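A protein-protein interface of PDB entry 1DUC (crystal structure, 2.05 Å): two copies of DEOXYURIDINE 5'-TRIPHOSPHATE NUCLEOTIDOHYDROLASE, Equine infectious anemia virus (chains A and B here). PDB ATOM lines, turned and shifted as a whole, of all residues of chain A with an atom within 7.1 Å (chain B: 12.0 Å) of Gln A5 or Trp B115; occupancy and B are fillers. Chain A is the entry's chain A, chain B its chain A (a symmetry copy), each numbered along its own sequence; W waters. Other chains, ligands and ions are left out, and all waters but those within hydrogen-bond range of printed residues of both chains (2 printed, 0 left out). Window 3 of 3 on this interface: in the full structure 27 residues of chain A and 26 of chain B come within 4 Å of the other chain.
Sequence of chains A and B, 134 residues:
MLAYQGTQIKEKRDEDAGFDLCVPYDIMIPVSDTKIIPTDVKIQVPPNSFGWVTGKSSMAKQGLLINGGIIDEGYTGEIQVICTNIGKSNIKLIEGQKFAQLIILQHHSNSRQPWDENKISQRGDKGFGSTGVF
The backbone carbonyl oxygen (O) of Ala A3 lies within hydrogen-bond range of the backbone NH (N) of Gln A44. N of Gln A5 sits at hydrogen-bond distance from O of Lys A42 (2.9 Å). The side-chain amide nitrogen of Gln B113 is in hydrogen-bond range of the backbone carbonyl oxygen of Ser B111 (2.7 Å).
Among the printed residues, merely in contact across the chains: Leu A2 with Asn B110, Leu A2 with Ser B111, Leu A2 with Arg B112, Ala A3 with Gln B113, Ala A3 with Pro B114, Ala A3 with Trp B115, Tyr A4 with Trp B115, Gln A5 with Trp B115, Lys A42 with Trp B115 and Ile A43 with Trp B115.
Hydrophobic or aromatic side chains of chain B that line the printed part of chain A: Trp B115. Of the 17 printed residues of chain A, 7 touch a printed residue of chain B. Hydrophobic or aromatic side chains of chain A within 4 Å of the printed part of chain B: Leu A2, Ala A3 and Tyr A4. Among the printed residues, 14 pairs touch across the chains.
No position is printed for both chains. Of the 14 pairs that touch across the chains among the printed residues, none has its exchanged pair printed and touching as well.
Of chain B, only Trp B115 (3.5 Å) comes within 4 Å of Gln A5. Thr A7 touches none of the printed residues of chain B. No residue of chain B comes within 4 Å of Ile A9. Val A41 touches none of the printed residues of chain B. Ile A43 touches just one residue of chain B: Trp B115 (3.9 Å). Of the printed residues of chain B, Gln A44 touches Trp B115 (3.1 Å) and Asp B116 (2.7 Å). Tyr A75 touches none of the printed residues of chain B. Of the printed residues of chain A, Ser B111 touches Leu A2 (3.8 Å). Of chain A, only Ala A3 (3.8 Å), Tyr A4 (3.8 Å), Gln A5 (3.5 Å), Lys A42 (3.5 Å), Ile A43 (3.9 Å) and Gln A44 (3.1 Å) come within 4 Å of Trp B115. Of the printed residues of chain A, Asp B116 touches Gln A44. The nearest residue of chain A that does not touch Trp B115 is Thr A76 (6.1 Å). The nearest printed residue of chain A that does not touch Ser B111 is Ala A3 (6.0 Å).
The backbone NH of Gln B113 lies within hydrogen-bond range of the backbone carbonyl oxygen of Leu A2. The backbone carbonyl oxygen (O) of Tyr A4 is in hydrogen-bond range of the guanidinium group (NH2) of Arg B112, at 3.0 Å. The side-chain amide nitrogen of Gln A44 lies close to the indole nitrogen of Trp B115, 3.4 Å away. The side-chain amide oxygen of Gln A44 is in hydrogen-bond range of the backbone NH of Asp B116 (2.7 Å).
Water W1 lies within hydrogen-bond range of the side-chain amide oxygen (OE1) of Gln A44 (2.5 Å), the backbone NH (N) of Asp B116 (3.5 Å) and the backbone carbonyl oxygen (O) of Pro B114 (3.5 Å). Water W2 lies within hydrogen-bond range of the backbone carbonyl oxygen of Gln B113 (2.5 Å), the guanidinium group of Arg B112 (2.9 Å) and the backbone NH of Tyr A4 (3.0 Å).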
ATOM      1  N   LEU A   2     -14.491   1.685  -0.785  1.00  0.00           N
ATOM      2  CA  LEU A   2     -14.302   0.806   0.357  1.00  0.00           C
ATOM      3  C   LEU A   2     -13.750   1.637   1.522  1.00  0.00           C
ATOM      4  O   LEU A   2     -13.262   2.732   1.236  1.00  0.00           O
ATOM      5  CB  LEU A   2     -13.291  -0.315   0.058  1.00  0.00           C
ATOM      6  CG  LEU A   2     -11.799  -0.009   0.120  1.00  0.00           C
ATOM      7  CD1 LEU A   2     -10.964  -1.288   0.070  1.00  0.00           C
ATOM      8  CD2 LEU A   2     -11.440   0.901  -1.067  1.00  0.00           C
ATOM      9  N   ALA A   3     -13.797   1.048   2.704  1.00  0.00           N
ATOM     10  CA  ALA A   3     -13.015   1.591   3.811  1.00  0.00           C
ATOM     11  C   ALA A   3     -12.003   0.501   4.157  1.00  0.00           C
ATOM     12  O   ALA A   3     -12.328  -0.701   4.001  1.00  0.00           O
ATOM     13  CB  ALA A   3     -13.946   1.883   5.013  1.00  0.00           C
ATOM     14  N   TYR A   4     -10.861   0.856   4.738  1.00  0.00           N
ATOM     15  CA  TYR A   4      -9.926  -0.171   5.183  1.00  0.00           C
ATOM     16  C   TYR A   4      -9.077   0.337   6.349  1.00  0.00           C
ATOM     17  O   TYR A   4      -8.934   1.550   6.502  1.00  0.00           O
ATOM     18  CB  TYR A   4      -8.947  -0.620   4.099  1.00  0.00           C
ATOM     19  CG  TYR A   4      -8.079   0.420   3.407  1.00  0.00           C
ATOM     20  CD1 TYR A   4      -6.840   0.790   3.889  1.00  0.00           C
ATOM     21  CD2 TYR A   4      -8.534   1.015   2.255  1.00  0.00           C
ATOM     22  CE1 TYR A   4      -6.053   1.734   3.250  1.00  0.00           C
ATOM     23  CE2 TYR A   4      -7.773   1.977   1.593  1.00  0.00           C
ATOM     24  CZ  TYR A   4      -6.538   2.308   2.099  1.00  0.00           C
ATOM     25  OH  TYR A   4      -5.790   3.249   1.434  1.00  0.00           O
ATOM     26  N   GLN A   5      -8.482  -0.611   7.053  1.00  0.00           N
ATOM     27  CA  GLN A   5      -7.560  -0.282   8.149  1.00  0.00           C
ATOM     28  C   GLN A   5      -6.419  -1.309   8.016  1.00  0.00           C
ATOM     29  O   GLN A   5      -6.680  -2.424   7.495  1.00  0.00           O
ATOM     30  CB  GLN A   5      -8.179  -0.578   9.502  1.00  0.00           C
ATOM     31  CG  GLN A   5      -9.447   0.087   9.948  1.00  0.00           C
ATOM     32  CD  GLN A   5      -9.811  -0.379  11.351  1.00  0.00           C
ATOM     33  OE1 GLN A   5      -9.642   0.389  12.290  1.00  0.00           O
ATOM     34  NE2 GLN A   5     -10.286  -1.609  11.467  1.00  0.00           N
ATOM     35  N   GLY A   6      -5.295  -0.993   8.621  1.00  0.00           N
ATOM     36  CA  GLY A   6      -4.171  -1.905   8.755  1.00  0.00           C
ATOM     37  C   GLY A   6      -2.884  -1.329   8.214  1.00  0.00           C
ATOM     38  O   GLY A   6      -2.877  -0.421   7.350  1.00  0.00           O
ATOM     39  N   THR A   7      -1.763  -1.891   8.618  1.00  0.00           N
ATOM     40  CA  THR A   7      -0.490  -1.314   8.138  1.00  0.00           C
ATOM     41  C   THR A   7      -0.004  -2.180   6.979  1.00  0.00           C
ATOM     42  O   THR A   7       0.911  -1.769   6.277  1.00  0.00           O
ATOM     43  CB  THR A   7       0.584  -1.461   9.255  1.00  0.00           C
ATOM     44  OG1 THR A   7       0.645  -2.843   9.632  1.00  0.00           O
ATOM     45  CG2 THR A   7       0.103  -0.682  10.510  1.00  0.00           C
ATOM     46  N   GLN A   8      -0.599  -3.367   6.727  1.00  0.00           N
ATOM     47  CA  GLN A   8      -0.028  -4.199   5.648  1.00  0.00           C
ATOM     48  C   GLN A   8      -0.704  -3.983   4.311  1.00  0.00           C
ATOM     49  O   GLN A   8      -0.750  -4.897   3.472  1.00  0.00           O
ATOM     50  CB  GLN A   8      -0.132  -5.691   6.037  1.00  0.00           C
ATOM     51  CG  GLN A   8       0.873  -6.006   7.183  1.00  0.00           C
ATOM     52  CD  GLN A   8       0.594  -7.434   7.628  1.00  0.00           C
ATOM     53  OE1 GLN A   8       0.110  -7.589   8.740  1.00  0.00           O
ATOM     54  NE2 GLN A   8       0.809  -8.492   6.814  1.00  0.00           N
ATOM     55  N   ILE A   9      -1.352  -2.868   4.088  1.00  0.00           N
ATOM     56  CA  ILE A   9      -2.001  -2.589   2.794  1.00  0.00           C
ATOM     57  C   ILE A   9      -1.385  -1.237   2.391  1.00  0.00           C
ATOM     58  O   ILE A   9      -1.303  -0.385   3.288  1.00  0.00           O
ATOM     59  CB  ILE A   9      -3.497  -2.570   2.901  1.00  0.00           C
ATOM     60  CG1 ILE A   9      -4.118  -2.015   1.602  1.00  0.00           C
ATOM     61  CG2 ILE A   9      -4.057  -1.675   4.053  1.00  0.00           C
ATOM     62  CD1 ILE A   9      -5.552  -2.482   1.436  1.00  0.00           C
ATOM     63  N   THR A  39      -2.529 -10.985   7.868  1.00  0.00           N
ATOM     64  CA  THR A  39      -2.340  -9.564   7.695  1.00  0.00           C
ATOM     65  C   THR A  39      -3.107  -8.908   8.848  1.00  0.00           C
ATOM     66  O   THR A  39      -4.039  -9.484   9.403  1.00  0.00           O
ATOM     67  CB  THR A  39      -2.810  -8.961   6.348  1.00  0.00           C
ATOM     68  OG1 THR A  39      -4.230  -8.865   6.375  1.00  0.00           O
ATOM     69  CG2 THR A  39      -2.308  -9.705   5.117  1.00  0.00           C
ATOM     70  N   ASP A  40      -2.915  -7.582   8.998  1.00  0.00           N
ATOM     71  CA  ASP A  40      -3.782  -6.864   9.943  1.00  0.00           C
ATOM     72  C   ASP A  40      -4.817  -6.093   9.168  1.00  0.00           C
ATOM     73  O   ASP A  40      -5.377  -5.077   9.638  1.00  0.00           O
ATOM     74  CB  ASP A  40      -2.903  -5.908  10.809  1.00  0.00           C
ATOM     75  CG  ASP A  40      -2.188  -4.900   9.931  1.00  0.00           C
ATOM     76  OD1 ASP A  40      -2.214  -4.908   8.654  1.00  0.00           O
ATOM     77  OD2 ASP A  40      -1.539  -3.988  10.528  1.00  0.00           O
ATOM     78  N   VAL A  41      -5.085  -6.475   7.915  1.00  0.00           N
ATOM     79  CA  VAL A  41      -5.947  -5.579   7.091  1.00  0.00           C
ATOM     80  C   VAL A  41      -7.415  -5.919   7.243  1.00  0.00           C
ATOM     81  O   VAL A  41      -7.787  -7.103   7.136  1.00  0.00           O
ATOM     82  CB  VAL A  41      -5.499  -5.727   5.622  1.00  0.00           C
ATOM     83  CG1 VAL A  41      -6.379  -4.912   4.676  1.00  0.00           C
ATOM     84  CG2 VAL A  41      -4.036  -5.268   5.493  1.00  0.00           C
ATOM     85  N   LYS A  42      -8.306  -4.955   7.441  1.00  0.00           N
ATOM     86  CA  LYS A  42      -9.740  -5.196   7.522  1.00  0.00           C
ATOM     87  C   LYS A  42     -10.409  -4.184   6.597  1.00  0.00           C
ATOM     88  O   LYS A  42      -9.814  -3.113   6.397  1.00  0.00           O
ATOM     89  CB  LYS A  42     -10.366  -4.921   8.889  1.00  0.00           C
ATOM     90  CG  LYS A  42      -9.695  -5.568  10.089  1.00  0.00           C
ATOM     91  CD  LYS A  42     -10.447  -5.029  11.339  1.00  0.00           C
ATOM     92  N   ILE A  43     -11.471  -4.639   5.916  1.00  0.00           N
ATOM     93  CA  ILE A  43     -12.058  -3.785   4.877  1.00  0.00           C
ATOM     94  C   ILE A  43     -13.564  -3.771   5.101  1.00  0.00           C
ATOM     95  O   ILE A  43     -14.121  -4.709   5.668  1.00  0.00           O
ATOM     96  CB  ILE A  43     -11.749  -4.281   3.443  1.00  0.00           C
ATOM     97  CG1 ILE A  43     -12.367  -5.713   3.257  1.00  0.00           C
ATOM     98  CG2 ILE A  43     -10.224  -4.402   3.194  1.00  0.00           C
ATOM     99  CD1 ILE A  43     -12.282  -6.157   1.777  1.00  0.00           C
ATOM    100  N   GLN A  44     -14.239  -2.737   4.636  1.00  0.00           N
ATOM    101  CA  GLN A  44     -15.680  -2.662   4.609  1.00  0.00           C
ATOM    102  C   GLN A  44     -16.076  -2.264   3.182  1.00  0.00           C
ATOM    103  O   GLN A  44     -15.566  -1.209   2.717  1.00  0.00           O
ATOM    104  CB  GLN A  44     -16.199  -1.461   5.513  1.00  0.00           C
ATOM    105  CG  GLN A  44     -15.921  -1.801   6.982  1.00  0.00           C
ATOM    106  CD  GLN A  44     -16.365  -0.740   7.986  1.00  0.00           C
ATOM    107  OE1 GLN A  44     -16.539   0.435   7.678  1.00  0.00           O
ATOM    108  NE2 GLN A  44     -16.541  -1.188   9.227  1.00  0.00           N
ATOM    109  N   TYR A  75     -17.662 -10.213   5.905  1.00  0.00           N
ATOM    110  CA  TYR A  75     -16.557 -10.647   6.820  1.00  0.00           C
ATOM    111  C   TYR A  75     -16.062  -9.499   7.670  1.00  0.00           C
ATOM    112  O   TYR A  75     -15.705  -8.452   7.102  1.00  0.00           O
ATOM    113  CB  TYR A  75     -15.401 -11.046   5.877  1.00  0.00           C
ATOM    114  CG  TYR A  75     -14.187 -11.614   6.570  1.00  0.00           C
ATOM    115  CD1 TYR A  75     -14.267 -12.766   7.359  1.00  0.00           C
ATOM    116  CD2 TYR A  75     -12.969 -10.977   6.437  1.00  0.00           C
ATOM    117  CE1 TYR A  75     -13.138 -13.317   7.959  1.00  0.00           C
ATOM    118  CE2 TYR A  75     -11.824 -11.500   7.025  1.00  0.00           C
ATOM    119  CZ  TYR A  75     -11.937 -12.657   7.787  1.00  0.00           C
ATOM    120  OH  TYR A  75     -10.793 -13.178   8.350  1.00  0.00           O
ATOM    121  N   THR A  76     -15.912  -9.645   8.973  1.00  0.00           N
ATOM    122  CA  THR A  76     -15.382  -8.475   9.707  1.00  0.00           C
ATOM    123  C   THR A  76     -14.025  -8.816  10.298  1.00  0.00           C
ATOM    124  O   THR A  76     -13.520  -7.983  11.041  1.00  0.00           O
ATOM    125  CB  THR A  76     -16.311  -8.058  10.886  1.00  0.00           C
ATOM    126  OG1 THR A  76     -16.497  -9.253  11.644  1.00  0.00           O
ATOM    127  CG2 THR A  76     -17.657  -7.552  10.419  1.00  0.00           C
ATOM    128  N   GLY A  77     -13.367  -9.935   9.974  1.00  0.00           N
ATOM    129  CA  GLY A  77     -12.035 -10.175  10.488  1.00  0.00           C
ATOM    130  C   GLY A  77     -10.932  -9.533   9.665  1.00  0.00           C
ATOM    131  O   GLY A  77     -11.100  -8.784   8.695  1.00  0.00           O
ATOM    132  N   ASN B 110     -10.929   2.216  -5.266  1.00  0.00           N
ATOM    133  CA  ASN B 110     -10.646   3.667  -5.367  1.00  0.00           C
ATOM    134  C   ASN B 110     -11.670   4.303  -4.423  1.00  0.00           C
ATOM    135  O   ASN B 110     -12.428   3.595  -3.718  1.00  0.00           O
ATOM    136  CB  ASN B 110     -10.705   4.135  -6.837  1.00  0.00           C
ATOM    137  CG  ASN B 110      -9.454   3.934  -7.673  1.00  0.00           C
ATOM    138  OD1 ASN B 110      -8.362   3.802  -7.091  1.00  0.00           O
ATOM    139  ND2 ASN B 110      -9.449   3.888  -9.007  1.00  0.00           N
ATOM    140  N   SER B 111     -11.649   5.627  -4.225  1.00  0.00           N
ATOM    141  CA  SER B 111     -12.566   6.348  -3.361  1.00  0.00           C
ATOM    142  C   SER B 111     -12.726   5.747  -1.965  1.00  0.00           C
ATOM    143  O   SER B 111     -13.780   5.349  -1.467  1.00  0.00           O
ATOM    144  CB  SER B 111     -13.951   6.491  -3.974  1.00  0.00           C
ATOM    145  OG  SER B 111     -14.220   5.472  -4.910  1.00  0.00           O
ATOM    146  N   ARG B 112     -11.620   5.808  -1.243  1.00  0.00           N
ATOM    147  CA  ARG B 112     -11.492   5.291   0.105  1.00  0.00           C
ATOM    148  C   ARG B 112     -12.520   6.027   0.977  1.00  0.00           C
ATOM    149  O   ARG B 112     -12.720   7.230   0.782  1.00  0.00           O
ATOM    150  CB  ARG B 112     -10.091   5.499   0.689  1.00  0.00           C
ATOM    151  CG  ARG B 112      -9.934   5.058   2.140  1.00  0.00           C
ATOM    152  CD  ARG B 112      -8.538   5.338   2.714  1.00  0.00           C
ATOM    153  NE  ARG B 112      -8.405   4.638   4.010  1.00  0.00           N
ATOM    154  CZ  ARG B 112      -7.272   4.565   4.707  1.00  0.00           C
ATOM    155  NH1 ARG B 112      -6.182   5.166   4.214  1.00  0.00           N
ATOM    156  NH2 ARG B 112      -7.199   3.904   5.866  1.00  0.00           N
ATOM    157  N   GLN B 113     -13.175   5.359   1.917  1.00  0.00           N
ATOM    158  CA  GLN B 113     -14.217   5.993   2.713  1.00  0.00           C
ATOM    159  C   GLN B 113     -13.763   5.871   4.164  1.00  0.00           C
ATOM    160  O   GLN B 113     -12.840   5.144   4.529  1.00  0.00           O
ATOM    161  CB  GLN B 113     -15.589   5.332   2.637  1.00  0.00           C
ATOM    162  CG  GLN B 113     -16.112   5.139   1.230  1.00  0.00           C
ATOM    163  CD  GLN B 113     -16.406   6.503   0.615  1.00  0.00           C
ATOM    164  OE1 GLN B 113     -17.282   7.235   1.094  1.00  0.00           O
ATOM    165  NE2 GLN B 113     -15.689   6.879  -0.416  1.00  0.00           N
ATOM    166  N   PRO B 114     -14.432   6.643   4.994  1.00  0.00           N
ATOM    167  CA  PRO B 114     -14.218   6.587   6.427  1.00  0.00           C
ATOM    168  C   PRO B 114     -14.716   5.238   6.932  1.00  0.00           C
ATOM    169  O   PRO B 114     -15.764   4.785   6.518  1.00  0.00           O
ATOM    170  CB  PRO B 114     -15.090   7.723   7.034  1.00  0.00           C
ATOM    171  CG  PRO B 114     -16.125   7.928   5.952  1.00  0.00           C
ATOM    172  CD  PRO B 114     -15.518   7.561   4.618  1.00  0.00           C
ATOM    173  N   TRP B 115     -14.037   4.619   7.858  1.00  0.00           N
ATOM    174  CA  TRP B 115     -14.510   3.385   8.473  1.00  0.00           C
ATOM    175  C   TRP B 115     -15.786   3.561   9.263  1.00  0.00           C
ATOM    176  O   TRP B 115     -15.855   4.506  10.067  1.00  0.00           O
ATOM    177  CB  TRP B 115     -13.358   3.015   9.427  1.00  0.00           C
ATOM    178  CG  TRP B 115     -13.581   1.644   9.998  1.00  0.00           C
ATOM    179  CD1 TRP B 115     -14.165   1.331  11.195  1.00  0.00           C
ATOM    180  CD2 TRP B 115     -13.226   0.403   9.364  1.00  0.00           C
ATOM    181  NE1 TRP B 115     -14.185  -0.036  11.343  1.00  0.00           N
ATOM    182  CE2 TRP B 115     -13.617  -0.628  10.231  1.00  0.00           C
ATOM    183  CE3 TRP B 115     -12.603   0.078   8.160  1.00  0.00           C
ATOM    184  CZ2 TRP B 115     -13.416  -1.983   9.953  1.00  0.00           C
ATOM    185  CZ3 TRP B 115     -12.420  -1.270   7.888  1.00  0.00           C
ATOM    186  CH2 TRP B 115     -12.819  -2.289   8.748  1.00  0.00           C
ATOM    187  N   ASP B 116     -16.811   2.729   9.166  1.00  0.00           N
ATOM    188  CA  ASP B 116     -17.973   2.859  10.026  1.00  0.00           C
ATOM    189  C   ASP B 116     -17.801   1.928  11.230  1.00  0.00           C
ATOM    190  O   ASP B 116     -17.863   0.695  11.133  1.00  0.00           O
ATOM    191  CB  ASP B 116     -19.278   2.585   9.297  1.00  0.00           C
ATOM    192  N   GLU B 117     -17.638   2.542  12.404  1.00  0.00           N
ATOM    193  CA  GLU B 117     -17.544   1.829  13.672  1.00  0.00           C
ATOM    194  C   GLU B 117     -18.853   1.181  14.089  1.00  0.00           C
ATOM    195  O   GLU B 117     -18.778   0.249  14.895  1.00  0.00           O
ATOM    196  CB  GLU B 117     -17.045   2.808  14.749  1.00  0.00           C
ATOM    197  CG  GLU B 117     -15.549   3.123  14.653  1.00  0.00           C
ATOM    198  N   ASN B 118     -19.981   1.525  13.492  1.00  0.00           N
ATOM    199  CA  ASN B 118     -21.278   0.945  13.819  1.00  0.00           C
ATOM    200  C   ASN B 118     -21.249  -0.576  13.924  1.00  0.00           C
ATOM    201  O   ASN B 118     -22.349  -1.171  14.044  1.00  0.00           O
ATOM    202  CB  ASN B 118     -22.345   1.350  12.788  1.00  0.00           C
HETATM  203  O   HOH W   1     -17.550   1.850   5.895  1.00  0.00           O
HETATM  204  O   HOH W   2     -10.809   3.842   5.326  1.00  0.00           O
